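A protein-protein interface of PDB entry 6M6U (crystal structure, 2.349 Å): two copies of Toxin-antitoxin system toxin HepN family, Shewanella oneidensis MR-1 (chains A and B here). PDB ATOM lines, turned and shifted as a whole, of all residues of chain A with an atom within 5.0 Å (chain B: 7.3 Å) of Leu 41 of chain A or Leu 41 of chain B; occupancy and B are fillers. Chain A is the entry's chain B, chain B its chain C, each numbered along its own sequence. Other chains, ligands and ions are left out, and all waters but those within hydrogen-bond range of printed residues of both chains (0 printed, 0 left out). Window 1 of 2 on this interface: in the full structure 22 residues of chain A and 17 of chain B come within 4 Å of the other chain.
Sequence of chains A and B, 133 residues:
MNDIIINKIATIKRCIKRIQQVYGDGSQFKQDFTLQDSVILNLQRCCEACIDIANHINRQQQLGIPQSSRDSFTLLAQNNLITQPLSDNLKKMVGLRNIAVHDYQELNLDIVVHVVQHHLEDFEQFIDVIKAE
The side-chain carboxylate (OD2) of Asp 37 of chain A lies within hydrogen-bond range of the side-chain amide nitrogen (ND2) of Asn 42 of chain B (3.1 Å). The guanidinium group (NH1) of Arg 45 of chain A lies within salt-bridge range of the side-chain carboxylate (OD1) of Asp 37 of chain B (3.3 Å). The side-chain amide nitrogen (ND2) of Asn 42 of chain A sits at hydrogen-bond distance from the side-chain carboxylate (OD2) of Asp 37 of chain B (3.1 Å). The side-chain amide nitrogen (NE2) of Gln 44 of chain A lies within hydrogen-bond range of the side-chain amide oxygen (OE1) of Gln 44 of chain B, 2.8 Å away. The side-chain hydroxyl (OG) of Ser 38 of chain A sits at hydrogen-bond distance from the side-chain carboxylate (OD2) of Asp 37 of chain B (2.8 Å). OD2 of Asp 37 of chain A lies within hydrogen-bond range of OG of Ser 38 of chain B (2.6 Å). NE of Arg 45 of chain B is in hydrogen-bond range of O of Val 101 of chain A (3.0 Å). The side-chain carboxylate (OD1) of Asp 37 of chain A lies within salt-bridge range of the guanidinium group (NH1) of Arg 45 of chain B (3.4 Å).
O of Asn 42 of chain B sits at hydrogen-bond distance from SG of Cys 46 of chain B (3.3 Å). The backbone carbonyl oxygen (O) of Ser 38 of chain A is in hydrogen-bond range of the side-chain amide nitrogen (ND2) of Asn 42 of chain A, 2.9 Å away. OE1 of Glu 48 of chain B lies within hydrogen-bond range of NE2 of Gln 44 of chain B, 3.2 Å away. The backbone carbonyl oxygen (O) of Ser 38 of chain B lies within hydrogen-bond range of the side-chain amide nitrogen (ND2) of Asn 42 of chain B. The side-chain sulfur of Cys 15 of chain B sits at hydrogen-bond distance from the side-chain amide oxygen of Asn 42 of chain B, at 3.5 Å. The side-chain amide oxygen (OD1) of Asn 42 of chain B lies within hydrogen-bond range of the guanidinium group (NH1) of Arg 45 of chain B (3.1 Å).
Among the printed residues, merely in contact across the chains: Asp 37 of chain A with Leu 41 of chain B (3.4 Å), Ile 40 of chain A with Leu 41 of chain B (3.96 Å), Leu 41 of chain A with Asp 37 of chain B (3.6 Å), Leu 41 of chain A with Leu 41 of chain B (3.7 Å), Gln 44 of chain A with Val 101 of chain B (3.97 Å), Arg 45 of chain A with Tyr 104 of chain B (3.0 Å) and Val 101 of chain A with Gln 44 of chain B (3.6 Å).
Of chain B, only Asp 37 and Leu 41 come within 4 Å of Leu 41 of chain A. Leu 41 of chain B touches three residues of chain A. Printed residues of chain A within 4 Å of Ser 38 of chain B: Asp 37 (2.6 Å). Printed residues of chain A within 4 Å of Asn 42 of chain B: Asp 37 (3.1 Å). Leu 107 of chain B touches none of the printed residues of chain A. The nearest residue of chain B that does not touch Leu 41 of chain A is Gln 44 of chain B (4.1 Å). The nearest residue of chain A that does not touch Leu 41 of chain B is Val 101 of chain A (4.1 Å). The nearest printed residue of chain B that does not touch Ser 38 of chain A is Ser 38 of chain B (4.8 Å).
Of the 21 printed residues of chain B, 8 touch a printed residue of chain A. Printed residues of chain B that touch a printed residue of chain A: Asp 37, Ser 38, Leu 41, Asn 42, Gln 44, Arg 45, Val 101 and Tyr 104. Hydrophobic or aromatic side chains of chain B that line the printed part of chain A: Leu 41, Val 101 and Tyr 104.
Leu 41 of chain A touches its own counterpart, Leu 41 of chain B. Gln 44 of chain A touches its own counterpart, Gln 44 of chain B. Gln 44 of chain A touches Val 101 of chain B, and with the chains exchanged Val 101 of chain A touches Gln 44 of chain B. Val 101 of chain A touches Arg 45 of chain B, but with the chains exchanged Arg 45 of chain A does not touch Val 101 of chain B (5.4 Å). 11 positions are printed for both chains. Of the 15 pairs that touch across the chains among the printed residues, 12 have their exchanged pair printed and touching as well.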
ATOM      1  N   GLN A  36       2.702   5.703   4.151  1.00  0.00           N
ATOM      2  CA  GLN A  36       3.434   6.965   4.157  1.00  0.00           C
ATOM      3  C   GLN A  36       3.287   7.665   5.502  1.00  0.00           C
ATOM      4  O   GLN A  36       4.278   8.110   6.093  1.00  0.00           O
ATOM      5  CB  GLN A  36       2.946   7.857   3.013  1.00  0.00           C
ATOM      6  CG  GLN A  36       3.217   7.261   1.635  1.00  0.00           C
ATOM      7  CD  GLN A  36       2.338   7.849   0.552  1.00  0.00           C
ATOM      8  OE1 GLN A  36       1.947   9.011   0.615  1.00  0.00           O
ATOM      9  NE2 GLN A  36       2.023   7.041  -0.454  1.00  0.00           N
ATOM     10  N   ASP A  37       2.054   7.749   6.008  1.00  0.00           N
ATOM     11  CA  ASP A  37       1.805   8.316   7.330  1.00  0.00           C
ATOM     12  C   ASP A  37       2.685   7.663   8.391  1.00  0.00           C
ATOM     13  O   ASP A  37       3.289   8.349   9.224  1.00  0.00           O
ATOM     14  CB  ASP A  37       0.329   8.154   7.694  1.00  0.00           C
ATOM     15  CG  ASP A  37      -0.589   9.007   6.833  1.00  0.00           C
ATOM     16  OD1 ASP A  37      -0.093   9.926   6.146  1.00  0.00           O
ATOM     17  OD2 ASP A  37      -1.817   8.765   6.861  1.00  0.00           O
ATOM     18  N   SER A  38       2.782   6.331   8.366  1.00  0.00           N
ATOM     19  CA  SER A  38       3.522   5.625   9.407  1.00  0.00           C
ATOM     20  C   SER A  38       5.026   5.826   9.260  1.00  0.00           C
ATOM     21  O   SER A  38       5.740   5.950  10.262  1.00  0.00           O
ATOM     22  CB  SER A  38       3.175   4.138   9.385  1.00  0.00           C
ATOM     23  OG  SER A  38       3.904   3.445  10.381  1.00  0.00           O
ATOM     24  N   VAL A  39       5.530   5.844   8.026  1.00  0.00           N
ATOM     25  CA  VAL A  39       6.947   6.127   7.815  1.00  0.00           C
ATOM     26  C   VAL A  39       7.266   7.557   8.228  1.00  0.00           C
ATOM     27  O   VAL A  39       8.260   7.820   8.917  1.00  0.00           O
ATOM     28  CB  VAL A  39       7.337   5.864   6.349  1.00  0.00           C
ATOM     29  CG1 VAL A  39       8.728   6.419   6.059  1.00  0.00           C
ATOM     30  CG2 VAL A  39       7.274   4.368   6.038  1.00  0.00           C
ATOM     31  N   ILE A  40       6.416   8.501   7.826  1.00  0.00           N
ATOM     32  CA  ILE A  40       6.663   9.908   8.122  1.00  0.00           C
ATOM     33  C   ILE A  40       6.647  10.153   9.627  1.00  0.00           C
ATOM     34  O   ILE A  40       7.482  10.897  10.156  1.00  0.00           O
ATOM     35  CB  ILE A  40       5.641  10.788   7.378  1.00  0.00           C
ATOM     36  CG1 ILE A  40       5.945  10.788   5.874  1.00  0.00           C
ATOM     37  CG2 ILE A  40       5.622  12.199   7.945  1.00  0.00           C
ATOM     38  CD1 ILE A  40       4.874  11.447   5.028  1.00  0.00           C
ATOM     39  N   LEU A  41       5.722   9.511  10.344  1.00  0.00           N
ATOM     40  CA  LEU A  41       5.633   9.726  11.785  1.00  0.00           C
ATOM     41  C   LEU A  41       6.855   9.163  12.498  1.00  0.00           C
ATOM     42  O   LEU A  41       7.407   9.798  13.407  1.00  0.00           O
ATOM     43  CB  LEU A  41       4.353   9.107  12.340  1.00  0.00           C
ATOM     44  CG  LEU A  41       4.164   9.394  13.838  1.00  0.00           C
ATOM     45  CD1 LEU A  41       3.499  10.751  14.047  1.00  0.00           C
ATOM     46  CD2 LEU A  41       3.362   8.302  14.514  1.00  0.00           C
ATOM     47  N   ASN A  42       7.301   7.972  12.099  1.00  0.00           N
ATOM     48  CA  ASN A  42       8.479   7.400  12.733  1.00  0.00           C
ATOM     49  C   ASN A  42       9.761   8.118  12.320  1.00  0.00           C
ATOM     50  O   ASN A  42      10.735   8.101  13.078  1.00  0.00           O
ATOM     51  CB  ASN A  42       8.560   5.905  12.433  1.00  0.00           C
ATOM     52  CG  ASN A  42       7.607   5.088  13.292  1.00  0.00           C
ATOM     53  OD1 ASN A  42       7.797   4.963  14.507  1.00  0.00           O
ATOM     54  ND2 ASN A  42       6.573   4.528  12.667  1.00  0.00           N
ATOM     55  N   LEU A  43       9.787   8.756  11.146  1.00  0.00           N
ATOM     56  CA  LEU A  43      10.891   9.662  10.841  1.00  0.00           C
ATOM     57  C   LEU A  43      10.898  10.846  11.802  1.00  0.00           C
ATOM     58  O   LEU A  43      11.949  11.223  12.335  1.00  0.00           O
ATOM     59  CB  LEU A  43      10.798  10.149   9.397  1.00  0.00           C
ATOM     60  CG  LEU A  43      11.449   9.244   8.352  1.00  0.00           C
ATOM     61  CD1 LEU A  43      11.208   9.777   6.943  1.00  0.00           C
ATOM     62  CD2 LEU A  43      12.940   9.092   8.636  1.00  0.00           C
ATOM     63  N   GLN A  44       9.723  11.441  12.033  1.00  0.00           N
ATOM     64  CA  GLN A  44       9.614  12.550  12.974  1.00  0.00           C
ATOM     65  C   GLN A  44      10.101  12.144  14.359  1.00  0.00           C
ATOM     66  O   GLN A  44      10.869  12.872  14.999  1.00  0.00           O
ATOM     67  CB  GLN A  44       8.169  13.035  13.033  1.00  0.00           C
ATOM     68  CG  GLN A  44       7.896  14.016  14.155  1.00  0.00           C
ATOM     69  CD  GLN A  44       6.486  14.551  14.110  1.00  0.00           C
ATOM     70  OE1 GLN A  44       6.200  15.507  13.392  1.00  0.00           O
ATOM     71  NE2 GLN A  44       5.588  13.927  14.868  1.00  0.00           N
ATOM     72  N   ARG A  45       9.663  10.976  14.837  1.00  0.00           N
ATOM     73  CA  ARG A  45      10.089  10.498  16.149  1.00  0.00           C
ATOM     74  C   ARG A  45      11.597  10.288  16.194  1.00  0.00           C
ATOM     75  O   ARG A  45      12.245  10.605  17.200  1.00  0.00           O
ATOM     76  CB  ARG A  45       9.344   9.207  16.494  1.00  0.00           C
ATOM     77  CG  ARG A  45       7.855   9.416  16.721  1.00  0.00           C
ATOM     78  CD  ARG A  45       7.096   8.116  16.793  1.00  0.00           C
ATOM     79  NE  ARG A  45       5.754   8.334  17.351  1.00  0.00           N
ATOM     80  CZ  ARG A  45       4.768   7.430  17.368  1.00  0.00           C
ATOM     81  NH1 ARG A  45       4.969   6.230  16.850  1.00  0.00           N
ATOM     82  NH2 ARG A  45       3.604   7.745  17.921  1.00  0.00           N
ATOM     83  N   VAL A 101       5.528  16.402   7.299  1.00  0.00           N
ATOM     84  CA  VAL A 101       4.473  16.509   8.299  1.00  0.00           C
ATOM     85  C   VAL A 101       3.566  17.702   8.016  1.00  0.00           C
ATOM     86  O   VAL A 101       2.339  17.564   7.965  1.00  0.00           O
ATOM     87  CB  VAL A 101       5.081  16.581   9.712  1.00  0.00           C
ATOM     88  CG1 VAL A 101       3.980  16.720  10.750  1.00  0.00           C
ATOM     89  CG2 VAL A 101       5.929  15.345   9.987  1.00  0.00           C
ATOM     90  N   CYS B  15      -7.282  15.644   6.376  1.00  0.00           N
ATOM     91  CA  CYS B  15      -6.751  14.856   7.478  1.00  0.00           C
ATOM     92  C   CYS B  15      -7.862  14.259   8.328  1.00  0.00           C
ATOM     93  O   CYS B  15      -7.703  13.154   8.860  1.00  0.00           O
ATOM     94  CB  CYS B  15      -5.824  15.711   8.341  1.00  0.00           C
ATOM     95  SG  CYS B  15      -4.263  16.126   7.538  1.00  0.00           S
ATOM     96  N   ILE B  19      -8.338  10.206   8.894  1.00  0.00           N
ATOM     97  CA  ILE B  19      -8.479   9.575  10.202  1.00  0.00           C
ATOM     98  C   ILE B  19      -9.704   8.669  10.227  1.00  0.00           C
ATOM     99  O   ILE B  19      -9.626   7.505  10.639  1.00  0.00           O
ATOM    100  CB  ILE B  19      -8.540  10.649  11.303  1.00  0.00           C
ATOM    101  CG1 ILE B  19      -7.166  11.297  11.479  1.00  0.00           C
ATOM    102  CG2 ILE B  19      -9.041  10.052  12.611  1.00  0.00           C
ATOM    103  CD1 ILE B  19      -7.164  12.488  12.409  1.00  0.00           C
ATOM    104  N   PHE B  33      -0.158  -1.266  14.799  1.00  0.00           N
ATOM    105  CA  PHE B  33       0.597  -0.050  15.090  1.00  0.00           C
ATOM    106  C   PHE B  33       0.572   0.919  13.917  1.00  0.00           C
ATOM    107  O   PHE B  33       0.632   2.138  14.117  1.00  0.00           O
ATOM    108  CB  PHE B  33       2.045  -0.393  15.446  1.00  0.00           C
ATOM    109  CG  PHE B  33       2.195  -1.197  16.705  1.00  0.00           C
ATOM    110  CD1 PHE B  33       1.172  -1.253  17.640  1.00  0.00           C
ATOM    111  CD2 PHE B  33       3.367  -1.894  16.958  1.00  0.00           C
ATOM    112  CE1 PHE B  33       1.314  -1.995  18.800  1.00  0.00           C
ATOM    113  CE2 PHE B  33       3.514  -2.637  18.116  1.00  0.00           C
ATOM    114  CZ  PHE B  33       2.487  -2.686  19.038  1.00  0.00           C
ATOM    115  N   LEU B  35      -1.901   1.589  11.831  1.00  0.00           N
ATOM    116  CA  LEU B  35      -3.102   2.416  11.891  1.00  0.00           C
ATOM    117  C   LEU B  35      -3.010   3.449  13.008  1.00  0.00           C
ATOM    118  O   LEU B  35      -3.530   4.561  12.865  1.00  0.00           O
ATOM    119  CB  LEU B  35      -4.350   1.550  12.080  1.00  0.00           C
ATOM    120  CG  LEU B  35      -4.649   0.399  11.114  1.00  0.00           C
ATOM    121  CD1 LEU B  35      -5.672  -0.536  11.738  1.00  0.00           C
ATOM    122  CD2 LEU B  35      -5.148   0.903   9.765  1.00  0.00           C
ATOM    123  N   GLN B  36      -2.364   3.102  14.124  1.00  0.00           N
ATOM    124  CA  GLN B  36      -2.137   4.079  15.184  1.00  0.00           C
ATOM    125  C   GLN B  36      -1.271   5.229  14.686  1.00  0.00           C
ATOM    126  O   GLN B  36      -1.599   6.402  14.893  1.00  0.00           O
ATOM    127  CB  GLN B  36      -1.498   3.399  16.398  1.00  0.00           C
ATOM    128  CG  GLN B  36      -2.423   2.435  17.122  1.00  0.00           C
ATOM    129  CD  GLN B  36      -1.682   1.492  18.049  1.00  0.00           C
ATOM    130  OE1 GLN B  36      -0.587   1.797  18.520  1.00  0.00           O
ATOM    131  NE2 GLN B  36      -2.276   0.335  18.314  1.00  0.00           N
ATOM    132  N   ASP B  37      -0.165   4.906  14.009  1.00  0.00           N
ATOM    133  CA  ASP B  37       0.720   5.941  13.480  1.00  0.00           C
ATOM    134  C   ASP B  37      -0.028   6.894  12.554  1.00  0.00           C
ATOM    135  O   ASP B  37       0.080   8.119  12.684  1.00  0.00           O
ATOM    136  CB  ASP B  37       1.892   5.297  12.739  1.00  0.00           C
ATOM    137  CG  ASP B  37       2.836   4.550  13.664  1.00  0.00           C
ATOM    138  OD1 ASP B  37       2.771   4.768  14.892  1.00  0.00           O
ATOM    139  OD2 ASP B  37       3.652   3.751  13.153  1.00  0.00           O
ATOM    140  N   SER B  38      -0.795   6.346  11.608  1.00  0.00           N
ATOM    141  CA  SER B  38      -1.460   7.185  10.617  1.00  0.00           C
ATOM    142  C   SER B  38      -2.462   8.126  11.267  1.00  0.00           C
ATOM    143  O   SER B  38      -2.522   9.313  10.924  1.00  0.00           O
ATOM    144  CB  SER B  38      -2.152   6.314   9.567  1.00  0.00           C
ATOM    145  OG  SER B  38      -2.780   7.117   8.582  1.00  0.00           O
ATOM    146  N   VAL B  39      -3.265   7.613  12.204  1.00  0.00           N
ATOM    147  CA  VAL B  39      -4.265   8.447  12.864  1.00  0.00           C
ATOM    148  C   VAL B  39      -3.589   9.499  13.732  1.00  0.00           C
ATOM    149  O   VAL B  39      -3.939  10.685  13.692  1.00  0.00           O
ATOM    150  CB  VAL B  39      -5.229   7.573  13.686  1.00  0.00           C
ATOM    151  CG1 VAL B  39      -6.009   8.431  14.680  1.00  0.00           C
ATOM    152  CG2 VAL B  39      -6.179   6.822  12.757  1.00  0.00           C
ATOM    153  N   ILE B  40      -2.612   9.078  14.537  1.00  0.00           N
ATOM    154  CA  ILE B  40      -1.905  10.014  15.402  1.00  0.00           C
ATOM    155  C   ILE B  40      -1.251  11.117  14.578  1.00  0.00           C
ATOM    156  O   ILE B  40      -1.337  12.299  14.926  1.00  0.00           O
ATOM    157  CB  ILE B  40      -0.881   9.262  16.271  1.00  0.00           C
ATOM    158  CG1 ILE B  40      -1.601   8.384  17.295  1.00  0.00           C
ATOM    159  CG2 ILE B  40       0.061  10.243  16.959  1.00  0.00           C
ATOM    160  CD1 ILE B  40      -0.704   7.364  17.972  1.00  0.00           C
ATOM    161  N   LEU B  41      -0.605  10.754  13.465  1.00  0.00           N
ATOM    162  CA  LEU B  41       0.026  11.767  12.621  1.00  0.00           C
ATOM    163  C   LEU B  41      -0.996  12.774  12.113  1.00  0.00           C
ATOM    164  O   LEU B  41      -0.790  13.990  12.213  1.00  0.00           O
ATOM    165  CB  LEU B  41       0.750  11.115  11.447  1.00  0.00           C
ATOM    166  CG  LEU B  41       1.416  12.130  10.510  1.00  0.00           C
ATOM    167  CD1 LEU B  41       2.518  12.888  11.230  1.00  0.00           C
ATOM    168  CD2 LEU B  41       1.962  11.457   9.259  1.00  0.00           C
ATOM    169  N   ASN B  42      -2.114  12.286  11.570  1.00  0.00           N
ATOM    170  CA  ASN B  42      -3.110  13.196  11.012  1.00  0.00           C
ATOM    171  C   ASN B  42      -3.835  13.984  12.096  1.00  0.00           C
ATOM    172  O   ASN B  42      -4.321  15.090  11.830  1.00  0.00           O
ATOM    173  CB  ASN B  42      -4.102  12.424  10.147  1.00  0.00           C
ATOM    174  CG  ASN B  42      -3.514  12.024   8.814  1.00  0.00           C
ATOM    175  OD1 ASN B  42      -3.039  12.870   8.052  1.00  0.00           O
ATOM    176  ND2 ASN B  42      -3.531  10.727   8.527  1.00  0.00           N
ATOM    177  N   LEU B  43      -3.930  13.439  13.312  1.00  0.00           N
ATOM    178  CA  LEU B  43      -4.382  14.244  14.445  1.00  0.00           C
ATOM    179  C   LEU B  43      -3.426  15.401  14.696  1.00  0.00           C
ATOM    180  O   LEU B  43      -3.851  16.549  14.871  1.00  0.00           O
ATOM    181  CB  LEU B  43      -4.510  13.377  15.698  1.00  0.00           C
ATOM    182  CG  LEU B  43      -5.841  12.659  15.905  1.00  0.00           C
ATOM    183  CD1 LEU B  43      -5.782  11.777  17.141  1.00  0.00           C
ATOM    184  CD2 LEU B  43      -6.956  13.679  16.021  1.00  0.00           C
ATOM    185  N   GLN B  44      -2.124  15.112  14.718  1.00  0.00           N
ATOM    186  CA  GLN B  44      -1.126  16.163  14.884  1.00  0.00           C
ATOM    187  C   GLN B  44      -1.252  17.219  13.793  1.00  0.00           C
ATOM    188  O   GLN B  44      -1.212  18.420  14.081  1.00  0.00           O
ATOM    189  CB  GLN B  44       0.279  15.551  14.889  1.00  0.00           C
ATOM    190  CG  GLN B  44       1.415  16.564  14.865  1.00  0.00           C
ATOM    191  CD  GLN B  44       2.782  15.920  14.679  1.00  0.00           C
ATOM    192  OE1 GLN B  44       2.942  14.705  14.840  1.00  0.00           O
ATOM    193  NE2 GLN B  44       3.772  16.731  14.328  1.00  0.00           N
ATOM    194  N   ARG B  45      -1.425  16.793  12.535  1.00  0.00           N
ATOM    195  CA  ARG B  45      -1.535  17.749  11.435  1.00  0.00           C
ATOM    196  C   ARG B  45      -2.757  18.647  11.591  1.00  0.00           C
ATOM    197  O   ARG B  45      -2.691  19.848  11.303  1.00  0.00           O
ATOM    198  CB  ARG B  45      -1.597  17.015  10.097  1.00  0.00           C
ATOM    199  CG  ARG B  45      -0.281  16.433   9.609  1.00  0.00           C
ATOM    200  CD  ARG B  45      -0.546  15.476   8.461  1.00  0.00           C
ATOM    201  NE  ARG B  45       0.656  15.138   7.707  1.00  0.00           N
ATOM    202  CZ  ARG B  45       0.759  14.068   6.920  1.00  0.00           C
ATOM    203  NH1 ARG B  45      -0.269  13.231   6.802  1.00  0.00           N
ATOM    204  NH2 ARG B  45       1.885  13.825   6.259  1.00  0.00           N
ATOM    205  N   CYS B  46      -3.892  18.074  12.009  1.00  0.00           N
ATOM    206  CA  CYS B  46      -5.081  18.881  12.269  1.00  0.00           C
ATOM    207  C   CYS B  46      -4.797  19.928  13.335  1.00  0.00           C
ATOM    208  O   CYS B  46      -5.128  21.109  13.174  1.00  0.00           O
ATOM    209  CB  CYS B  46      -6.243  17.987  12.710  1.00  0.00           C
ATOM    210  SG  CYS B  46      -7.008  16.981  11.422  1.00  0.00           S
ATOM    211  N   CYS B  47      -4.179  19.503  14.437  1.00  0.00           N
ATOM    212  CA  CYS B  47      -3.869  20.424  15.521  1.00  0.00           C
ATOM    213  C   CYS B  47      -2.936  21.532  15.045  1.00  0.00           C
ATOM    214  O   CYS B  47      -3.188  22.717  15.288  1.00  0.00           O
ATOM    215  CB  CYS B  47      -3.255  19.656  16.689  1.00  0.00           C
ATOM    216  SG  CYS B  47      -2.987  20.664  18.141  1.00  0.00           S
ATOM    217  N   GLU B  48      -1.865  21.166  14.341  1.00  0.00           N
ATOM    218  CA  GLU B  48      -0.880  22.162  13.929  1.00  0.00           C
ATOM    219  C   GLU B  48      -1.401  23.057  12.809  1.00  0.00           C
ATOM    220  O   GLU B  48      -1.024  24.234  12.738  1.00  0.00           O
ATOM    221  CB  GLU B  48       0.426  21.465  13.539  1.00  0.00           C
ATOM    222  CG  GLU B  48       0.918  20.534  14.648  1.00  0.00           C
ATOM    223  CD  GLU B  48       2.322  19.997  14.450  1.00  0.00           C
ATOM    224  OE1 GLU B  48       2.954  19.571  15.444  1.00  0.00           O
ATOM    225  OE2 GLU B  48       2.813  19.992  13.305  1.00  0.00           O
ATOM    226  N   ALA B 100       2.447  13.510  21.697  1.00  0.00           N
ATOM    227  CA  ALA B 100       2.701  12.694  20.512  1.00  0.00           C
ATOM    228  C   ALA B 100       4.038  13.042  19.860  1.00  0.00           C
ATOM    229  O   ALA B 100       4.727  12.159  19.336  1.00  0.00           O
ATOM    230  CB  ALA B 100       1.562  12.859  19.506  1.00  0.00           C
ATOM    231  N   VAL B 101       4.426  14.318  19.887  1.00  0.00           N
ATOM    232  CA  VAL B 101       5.633  14.743  19.184  1.00  0.00           C
ATOM    233  C   VAL B 101       6.874  14.527  20.043  1.00  0.00           C
ATOM    234  O   VAL B 101       7.907  14.044  19.559  1.00  0.00           O
ATOM    235  CB  VAL B 101       5.503  16.214  18.742  1.00  0.00           C
ATOM    236  CG1 VAL B 101       6.809  16.708  18.135  1.00  0.00           C
ATOM    237  CG2 VAL B 101       4.361  16.372  17.751  1.00  0.00           C
ATOM    238  N   TYR B 104       6.265  10.068  22.410  1.00  0.00           N
ATOM    239  CA  TYR B 104       5.122   9.370  21.830  1.00  0.00           C
ATOM    240  C   TYR B 104       4.741   8.126  22.617  1.00  0.00           C
ATOM    241  O   TYR B 104       3.573   7.723  22.604  1.00  0.00           O
ATOM    242  CB  TYR B 104       5.431   8.986  20.390  1.00  0.00           C
ATOM    243  CG  TYR B 104       6.389   7.815  20.262  1.00  0.00           C
ATOM    244  CD1 TYR B 104       5.914   6.511  20.126  1.00  0.00           C
ATOM    245  CD2 TYR B 104       7.766   8.013  20.269  1.00  0.00           C
ATOM    246  CE1 TYR B 104       6.780   5.446  20.000  1.00  0.00           C
ATOM    247  CE2 TYR B 104       8.638   6.947  20.145  1.00  0.00           C
ATOM    248  CZ  TYR B 104       8.139   5.666  20.013  1.00  0.00           C
ATOM    249  OH  TYR B 104       8.999   4.598  19.891  1.00  0.00           O
ATOM    250  N   LEU B 107       1.684   8.230  24.957  1.00  0.00           N
ATOM    251  CA  LEU B 107       0.331   8.461  24.478  1.00  0.00           C
ATOM    252  C   LEU B 107      -0.605   7.398  25.035  1.00  0.00           C
ATOM    253  O   LEU B 107      -0.268   6.211  25.083  1.00  0.00           O
ATOM    254  CB  LEU B 107       0.289   8.444  22.949  1.00  0.00           C
ATOM    255  CG  LEU B 107       0.788   9.678  22.198  1.00  0.00           C
ATOM    256  CD1 LEU B 107       0.802   9.411  20.701  1.00  0.00           C
ATOM    257  CD2 LEU B 107      -0.084  10.880  22.519  1.00  0.00           C
